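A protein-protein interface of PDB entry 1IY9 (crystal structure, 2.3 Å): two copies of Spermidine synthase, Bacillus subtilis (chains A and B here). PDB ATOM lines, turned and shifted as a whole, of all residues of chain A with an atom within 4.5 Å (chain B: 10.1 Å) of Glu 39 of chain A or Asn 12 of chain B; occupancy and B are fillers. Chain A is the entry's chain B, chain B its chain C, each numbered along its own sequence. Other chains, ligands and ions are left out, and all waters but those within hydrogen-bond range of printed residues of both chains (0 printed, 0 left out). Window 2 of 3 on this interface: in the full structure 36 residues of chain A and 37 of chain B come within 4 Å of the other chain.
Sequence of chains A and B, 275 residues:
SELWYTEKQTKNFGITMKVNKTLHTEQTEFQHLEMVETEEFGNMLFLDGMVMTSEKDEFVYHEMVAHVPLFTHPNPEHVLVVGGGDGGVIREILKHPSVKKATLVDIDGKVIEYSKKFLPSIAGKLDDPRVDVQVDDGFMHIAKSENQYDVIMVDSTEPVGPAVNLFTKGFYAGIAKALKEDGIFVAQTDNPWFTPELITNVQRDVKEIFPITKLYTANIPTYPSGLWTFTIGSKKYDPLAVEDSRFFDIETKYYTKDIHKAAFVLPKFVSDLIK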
ATOM      1  N   TRP A   4       2.576  -0.510  -2.982  1.00  0.00           N
ATOM      2  CA  TRP A   4       3.622  -1.520  -2.855  1.00  0.00           C
ATOM      3  C   TRP A   4       4.116  -1.975  -4.197  1.00  0.00           C
ATOM      4  O   TRP A   4       3.348  -2.103  -5.136  1.00  0.00           O
ATOM      5  CB  TRP A   4       3.105  -2.763  -2.104  1.00  0.00           C
ATOM      6  CG  TRP A   4       2.800  -2.522  -0.672  1.00  0.00           C
ATOM      7  CD1 TRP A   4       1.795  -1.762  -0.186  1.00  0.00           C
ATOM      8  CD2 TRP A   4       3.555  -2.981   0.471  1.00  0.00           C
ATOM      9  NE1 TRP A   4       1.878  -1.697   1.189  1.00  0.00           N
ATOM     10  CE2 TRP A   4       2.945  -2.435   1.619  1.00  0.00           C
ATOM     11  CE3 TRP A   4       4.676  -3.790   0.631  1.00  0.00           C
ATOM     12  CZ2 TRP A   4       3.424  -2.661   2.913  1.00  0.00           C
ATOM     13  CZ3 TRP A   4       5.154  -4.018   1.929  1.00  0.00           C
ATOM     14  CH2 TRP A   4       4.530  -3.457   3.046  1.00  0.00           C
ATOM     15  N   THR A  16       7.807  -7.894  -1.532  1.00  0.00           N
ATOM     16  CA  THR A  16       6.970  -6.735  -1.742  1.00  0.00           C
ATOM     17  C   THR A  16       7.506  -5.607  -0.843  1.00  0.00           C
ATOM     18  O   THR A  16       7.766  -5.821   0.342  1.00  0.00           O
ATOM     19  CB  THR A  16       5.454  -7.138  -1.534  1.00  0.00           C
ATOM     20  OG1 THR A  16       4.577  -6.046  -1.877  1.00  0.00           O
ATOM     21  CG2 THR A  16       5.191  -7.621  -0.095  1.00  0.00           C
ATOM     22  N   MET A  17       7.843  -4.483  -1.484  1.00  0.00           N
ATOM     23  CA  MET A  17       8.403  -3.273  -0.834  1.00  0.00           C
ATOM     24  C   MET A  17       7.377  -2.141  -0.785  1.00  0.00           C
ATOM     25  O   MET A  17       6.735  -1.840  -1.790  1.00  0.00           O
ATOM     26  CB  MET A  17       9.612  -2.710  -1.632  1.00  0.00           C
ATOM     27  CG  MET A  17      10.953  -3.422  -1.558  1.00  0.00           C
ATOM     28  SD  MET A  17      11.195  -4.933  -2.514  1.00  0.00           S
ATOM     29  CE  MET A  17      10.558  -4.595  -3.978  1.00  0.00           C
ATOM     30  N   LYS A  18       7.268  -1.471   0.358  1.00  0.00           N
ATOM     31  CA  LYS A  18       6.362  -0.331   0.464  1.00  0.00           C
ATOM     32  C   LYS A  18       7.044   0.892  -0.164  1.00  0.00           C
ATOM     33  O   LYS A  18       8.192   1.246   0.196  1.00  0.00           O
ATOM     34  CB  LYS A  18       6.019  -0.022   1.905  1.00  0.00           C
ATOM     35  CG  LYS A  18       4.744   0.782   2.023  1.00  0.00           C
ATOM     36  CD  LYS A  18       4.735   1.584   3.280  1.00  0.00           C
ATOM     37  CE  LYS A  18       3.478   2.437   3.357  1.00  0.00           C
ATOM     38  NZ  LYS A  18       2.369   1.537   3.708  1.00  0.00           N
ATOM     39  N   ASN A  20       7.072   5.009  -1.246  1.00  0.00           N
ATOM     40  CA  ASN A  20       6.601   6.323  -0.828  1.00  0.00           C
ATOM     41  C   ASN A  20       6.212   7.187  -2.017  1.00  0.00           C
ATOM     42  O   ASN A  20       5.277   7.982  -1.938  1.00  0.00           O
ATOM     43  CB  ASN A  20       7.649   7.016   0.015  1.00  0.00           C
ATOM     44  CG  ASN A  20       7.744   6.430   1.386  1.00  0.00           C
ATOM     45  OD1 ASN A  20       6.791   5.856   1.902  1.00  0.00           O
ATOM     46  ND2 ASN A  20       8.902   6.550   1.985  1.00  0.00           N
ATOM     47  N   GLU A  37      11.290   5.488  -4.459  1.00  0.00           N
ATOM     48  CA  GLU A  37      11.752   5.679  -3.108  1.00  0.00           C
ATOM     49  C   GLU A  37      11.006   4.701  -2.195  1.00  0.00           C
ATOM     50  O   GLU A  37       9.784   4.808  -2.041  1.00  0.00           O
ATOM     51  CB  GLU A  37      11.501   7.095  -2.623  1.00  0.00           C
ATOM     52  CG  GLU A  37      11.931   7.250  -1.174  1.00  0.00           C
ATOM     53  CD  GLU A  37      11.382   8.503  -0.538  1.00  0.00           C
ATOM     54  OE1 GLU A  37      11.650   9.612  -1.060  1.00  0.00           O
ATOM     55  OE2 GLU A  37      10.671   8.386   0.485  1.00  0.00           O
ATOM     56  N   THR A  38      11.714   3.719  -1.644  1.00  0.00           N
ATOM     57  CA  THR A  38      11.063   2.777  -0.744  1.00  0.00           C
ATOM     58  C   THR A  38      11.291   3.195   0.697  1.00  0.00           C
ATOM     59  O   THR A  38      12.286   3.853   1.031  1.00  0.00           O
ATOM     60  CB  THR A  38      11.547   1.321  -0.928  1.00  0.00           C
ATOM     61  OG1 THR A  38      12.851   1.143  -0.352  1.00  0.00           O
ATOM     62  CG2 THR A  38      11.560   0.954  -2.408  1.00  0.00           C
ATOM     63  N   GLU A  39      10.370   2.801   1.563  1.00  0.00           N
ATOM     64  CA  GLU A  39      10.494   3.166   2.953  1.00  0.00           C
ATOM     65  C   GLU A  39      11.546   2.334   3.653  1.00  0.00           C
ATOM     66  O   GLU A  39      12.281   2.846   4.486  1.00  0.00           O
ATOM     67  CB  GLU A  39       9.138   3.049   3.655  1.00  0.00           C
ATOM     68  CG  GLU A  39       9.179   3.296   5.148  1.00  0.00           C
ATOM     69  CD  GLU A  39       9.662   4.694   5.535  1.00  0.00           C
ATOM     70  OE1 GLU A  39       9.488   5.649   4.727  1.00  0.00           O
ATOM     71  OE2 GLU A  39      10.211   4.826   6.666  1.00  0.00           O
ATOM     72  N   GLU A  40      11.660   1.071   3.252  1.00  0.00           N
ATOM     73  CA  GLU A  40      12.605   0.173   3.875  1.00  0.00           C
ATOM     74  C   GLU A  40      14.043   0.304   3.421  1.00  0.00           C
ATOM     75  O   GLU A  40      14.951   0.371   4.245  1.00  0.00           O
ATOM     76  CB  GLU A  40      12.139  -1.265   3.676  1.00  0.00           C
ATOM     77  CG  GLU A  40      12.937  -2.315   4.453  1.00  0.00           C
ATOM     78  CD  GLU A  40      12.946  -2.075   5.966  1.00  0.00           C
ATOM     79  OE1 GLU A  40      11.877  -1.841   6.567  1.00  0.00           O
ATOM     80  OE2 GLU A  40      14.033  -2.110   6.566  1.00  0.00           O
ATOM     81  N   PHE A  41      14.249   0.401   2.114  1.00  0.00           N
ATOM     82  CA  PHE A  41      15.607   0.442   1.585  1.00  0.00           C
ATOM     83  C   PHE A  41      16.116   1.740   0.974  1.00  0.00           C
ATOM     84  O   PHE A  41      17.228   1.777   0.432  1.00  0.00           O
ATOM     85  CB  PHE A  41      15.754  -0.666   0.549  1.00  0.00           C
ATOM     86  CG  PHE A  41      15.478  -2.027   1.084  1.00  0.00           C
ATOM     87  CD1 PHE A  41      14.236  -2.615   0.932  1.00  0.00           C
ATOM     88  CD2 PHE A  41      16.457  -2.718   1.767  1.00  0.00           C
ATOM     89  CE1 PHE A  41      13.984  -3.879   1.466  1.00  0.00           C
ATOM     90  CE2 PHE A  41      16.205  -3.975   2.295  1.00  0.00           C
ATOM     91  CZ  PHE A  41      14.970  -4.545   2.143  1.00  0.00           C
ATOM     92  N   THR B   6       0.923 -13.373   2.453  1.00  0.00           N
ATOM     93  CA  THR B   6       1.984 -12.389   2.612  1.00  0.00           C
ATOM     94  C   THR B   6       2.450 -12.237   4.051  1.00  0.00           C
ATOM     95  O   THR B   6       1.641 -12.265   4.970  1.00  0.00           O
ATOM     96  CB  THR B   6       1.534 -11.005   2.095  1.00  0.00           C
ATOM     97  OG1 THR B   6       1.240 -11.105   0.705  1.00  0.00           O
ATOM     98  CG2 THR B   6       2.632  -9.953   2.279  1.00  0.00           C
ATOM     99  N   GLU B   7       3.762 -12.161   4.249  1.00  0.00           N
ATOM    100  CA  GLU B   7       4.277 -11.920   5.579  1.00  0.00           C
ATOM    101  C   GLU B   7       5.020 -10.588   5.520  1.00  0.00           C
ATOM    102  O   GLU B   7       5.990 -10.418   4.753  1.00  0.00           O
ATOM    103  CB  GLU B   7       5.212 -13.031   6.095  1.00  0.00           C
ATOM    104  CG  GLU B   7       5.392 -12.916   7.604  1.00  0.00           C
ATOM    105  CD  GLU B   7       6.700 -13.457   8.125  1.00  0.00           C
ATOM    106  OE1 GLU B   7       7.153 -14.523   7.655  1.00  0.00           O
ATOM    107  OE2 GLU B   7       7.275 -12.805   9.029  1.00  0.00           O
ATOM    108  N   LYS B   8       4.480  -9.600   6.224  1.00  0.00           N
ATOM    109  CA  LYS B   8       5.124  -8.293   6.305  1.00  0.00           C
ATOM    110  C   LYS B   8       6.194  -8.488   7.371  1.00  0.00           C
ATOM    111  O   LYS B   8       5.944  -8.397   8.558  1.00  0.00           O
ATOM    112  CB  LYS B   8       4.139  -7.197   6.716  1.00  0.00           C
ATOM    113  CG  LYS B   8       3.048  -6.934   5.696  1.00  0.00           C
ATOM    114  CD  LYS B   8       3.636  -6.358   4.439  1.00  0.00           C
ATOM    115  CE  LYS B   8       2.625  -6.320   3.287  1.00  0.00           C
ATOM    116  NZ  LYS B   8       1.403  -5.517   3.566  1.00  0.00           N
ATOM    117  N   GLN B   9       7.382  -8.833   6.924  1.00  0.00           N
ATOM    118  CA  GLN B   9       8.511  -9.073   7.807  1.00  0.00           C
ATOM    119  C   GLN B   9       8.938  -7.784   8.484  1.00  0.00           C
ATOM    120  O   GLN B   9       9.712  -7.787   9.427  1.00  0.00           O
ATOM    121  CB  GLN B   9       9.667  -9.649   6.988  1.00  0.00           C
ATOM    122  CG  GLN B   9       9.287 -10.942   6.280  1.00  0.00           C
ATOM    123  CD  GLN B   9      10.296 -11.353   5.270  1.00  0.00           C
ATOM    124  OE1 GLN B   9      10.879 -10.517   4.579  1.00  0.00           O
ATOM    125  NE2 GLN B   9      10.525 -12.643   5.172  1.00  0.00           N
ATOM    126  N   THR B  10       8.391  -6.687   7.987  1.00  0.00           N
ATOM    127  CA  THR B  10       8.649  -5.336   8.459  1.00  0.00           C
ATOM    128  C   THR B  10       7.366  -4.626   8.031  1.00  0.00           C
ATOM    129  O   THR B  10       6.658  -5.126   7.171  1.00  0.00           O
ATOM    130  CB  THR B  10       9.823  -4.763   7.651  1.00  0.00           C
ATOM    131  OG1 THR B  10      11.055  -5.137   8.259  1.00  0.00           O
ATOM    132  CG2 THR B  10       9.745  -3.325   7.554  1.00  0.00           C
ATOM    133  N   LYS B  11       7.040  -3.488   8.622  1.00  0.00           N
ATOM    134  CA  LYS B  11       5.839  -2.763   8.198  1.00  0.00           C
ATOM    135  C   LYS B  11       5.947  -2.364   6.725  1.00  0.00           C
ATOM    136  O   LYS B  11       4.935  -2.218   6.044  1.00  0.00           O
ATOM    137  CB  LYS B  11       5.631  -1.494   9.045  1.00  0.00           C
ATOM    138  CG  LYS B  11       5.285  -1.777  10.494  1.00  0.00           C
ATOM    139  CD  LYS B  11       5.017  -0.524  11.313  1.00  0.00           C
ATOM    140  CE  LYS B  11       4.583  -0.917  12.744  1.00  0.00           C
ATOM    141  NZ  LYS B  11       4.169   0.259  13.592  1.00  0.00           N
ATOM    142  N   ASN B  12       7.180  -2.266   6.230  1.00  0.00           N
ATOM    143  CA  ASN B  12       7.463  -1.840   4.858  1.00  0.00           C
ATOM    144  C   ASN B  12       8.087  -2.853   3.906  1.00  0.00           C
ATOM    145  O   ASN B  12       8.527  -2.483   2.811  1.00  0.00           O
ATOM    146  CB  ASN B  12       8.401  -0.646   4.900  1.00  0.00           C
ATOM    147  CG  ASN B  12       7.957   0.412   5.868  1.00  0.00           C
ATOM    148  OD1 ASN B  12       6.896   1.003   5.706  1.00  0.00           O
ATOM    149  ND2 ASN B  12       8.784   0.677   6.888  1.00  0.00           N
ATOM    150  N   PHE B  13       8.144  -4.116   4.290  1.00  0.00           N
ATOM    151  CA  PHE B  13       8.775  -5.098   3.428  1.00  0.00           C
ATOM    152  C   PHE B  13       8.333  -6.492   3.834  1.00  0.00           C
ATOM    153  O   PHE B  13       8.098  -6.754   5.007  1.00  0.00           O
ATOM    154  CB  PHE B  13      10.296  -4.970   3.571  1.00  0.00           C
ATOM    155  CG  PHE B  13      11.074  -5.998   2.816  1.00  0.00           C
ATOM    156  CD1 PHE B  13      11.187  -5.923   1.436  1.00  0.00           C
ATOM    157  CD2 PHE B  13      11.741  -7.013   3.483  1.00  0.00           C
ATOM    158  CE1 PHE B  13      11.956  -6.837   0.724  1.00  0.00           C
ATOM    159  CE2 PHE B  13      12.516  -7.938   2.784  1.00  0.00           C
ATOM    160  CZ  PHE B  13      12.626  -7.847   1.401  1.00  0.00           C
ATOM    161  N   GLY B  14       8.243  -7.381   2.855  1.00  0.00           N
ATOM    162  CA  GLY B  14       7.851  -8.739   3.133  1.00  0.00           C
ATOM    163  C   GLY B  14       7.949  -9.659   1.937  1.00  0.00           C
ATOM    164  O   GLY B  14       8.398  -9.277   0.859  1.00  0.00           O
ATOM    165  N   ILE B  15       7.555 -10.904   2.147  1.00  0.00           N
ATOM    166  CA  ILE B  15       7.588 -11.895   1.102  1.00  0.00           C
ATOM    167  C   ILE B  15       6.155 -12.337   0.852  1.00  0.00           C
ATOM    168  O   ILE B  15       5.291 -12.215   1.737  1.00  0.00           O
ATOM    169  CB  ILE B  15       8.455 -13.103   1.492  1.00  0.00           C
ATOM    170  CG1 ILE B  15       8.048 -13.643   2.866  1.00  0.00           C
ATOM    171  CG2 ILE B  15       9.936 -12.725   1.450  1.00  0.00           C
ATOM    172  CD1 ILE B  15       8.667 -14.961   3.177  1.00  0.00           C
ATOM    173  N   PHE B 194      17.027  -6.032  10.038  1.00  0.00           N
ATOM    174  CA  PHE B 194      15.853  -5.349  10.565  1.00  0.00           C
ATOM    175  C   PHE B 194      15.746  -5.348  12.096  1.00  0.00           C
ATOM    176  O   PHE B 194      15.073  -4.497  12.693  1.00  0.00           O
ATOM    177  CB  PHE B 194      14.596  -5.954   9.925  1.00  0.00           C
ATOM    178  CG  PHE B 194      14.710  -6.186   8.418  1.00  0.00           C
ATOM    179  CD1 PHE B 194      14.396  -7.427   7.858  1.00  0.00           C
ATOM    180  CD2 PHE B 194      15.122  -5.169   7.565  1.00  0.00           C
ATOM    181  CE1 PHE B 194      14.493  -7.641   6.482  1.00  0.00           C
ATOM    182  CE2 PHE B 194      15.219  -5.384   6.183  1.00  0.00           C
ATOM    183  CZ  PHE B 194      14.902  -6.623   5.646  1.00  0.00           C
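N of Lys 18 of chain A sits at hydrogen-bond distance from O of Asn 12 of chain B. The backbone NH of Thr 16 of chain A sits at hydrogen-bond distance from the backbone carbonyl oxygen of Gly 14 of chain B, 2.8 Å away.
N of Phe 41 of chain A is in hydrogen-bond range of OG1 of Thr 38 of chain A (2.9 Å). OE1 of Glu 39 of chain A lies within hydrogen-bond range of ND2 of Asn 20 of chain A, 2.9 Å away. N of Glu 39 of chain A sits at hydrogen-bond distance from O of Lys 18 of chain A (3.0 Å).
Among the printed residues, pairs that only touch across the chains: Trp 4 of chain A with Lys 8 of chain B (3.3 Å), Trp 4 of chain A with Lys 11 of chain B (3.3 Å), Trp 4 of chain A with Asn 12 of chain B (3.7 Å), Trp 4 of chain A with Phe 13 of chain B (3.8 Å), Thr 16 of chain A with Phe 13 of chain B (3.3 Å), Met 17 of chain A with Asn 12 of chain B (3.7 Å), Met 17 of chain A with Phe 13 of chain B (3.8 Å), Glu 39 of chain A with Asn 12 of chain B (3.2 Å), Glu 40 of chain A with Thr 10 of chain B (2.8 Å), Glu 40 of chain A with Asn 12 of chain B (3.9 Å), Glu 40 of chain A with Phe 13 of chain B (3.8 Å), Glu 40 of chain A with Phe 194 of chain B (3.4 Å) and Phe 41 of chain A with Phe 13 of chain B (3.5 Å).
Glu 39 of chain A touches one residue of chain B. Of the printed residues of chain A, Asn 12 of chain B touches Trp 4, Met 17, Lys 18, Glu 39 and Glu 40. Printed residues of chain A within 4 Å of Phe 194 of chain B: Glu 40. Of the printed residues of chain A, Phe 13 of chain B touches Trp 4 (3.8 Å), Thr 16 (3.3 Å), Met 17 (3.8 Å), Glu 40 (3.8 Å) and Phe 41 (3.5 Å). Printed residues of chain B within 4 Å of Thr 16 of chain A: Phe 13 and Gly 14. Of the printed residues of chain A, Thr 10 of chain B touches Glu 40 (2.8 Å). Printed residues of chain B within 4 Å of Trp 4 of chain A: Lys 8 (3.3 Å), Lys 11 (3.3 Å), Asn 12 (3.7 Å) and Phe 13 (3.8 Å). The nearest residue of chain B that does not touch Glu 39 of chain A is Lys 11 of chain B (6.7 Å). The nearest residue of chain A that does not touch Asn 12 of chain B is Thr 16 of chain A (4.2 Å).
Along chain B the printed residues that touch a printed residue of chain A span positions 8 to 194. Of the 10 printed residues of chain A, 7 touch a printed residue of chain B. Printed residues of chain A that touch a printed residue of chain B: Trp 4, Thr 16, Met 17, Lys 18, Glu 39, Glu 40 and Phe 41. Among the printed residues, 15 pairs touch across the chains.
No position is printed for both chains.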
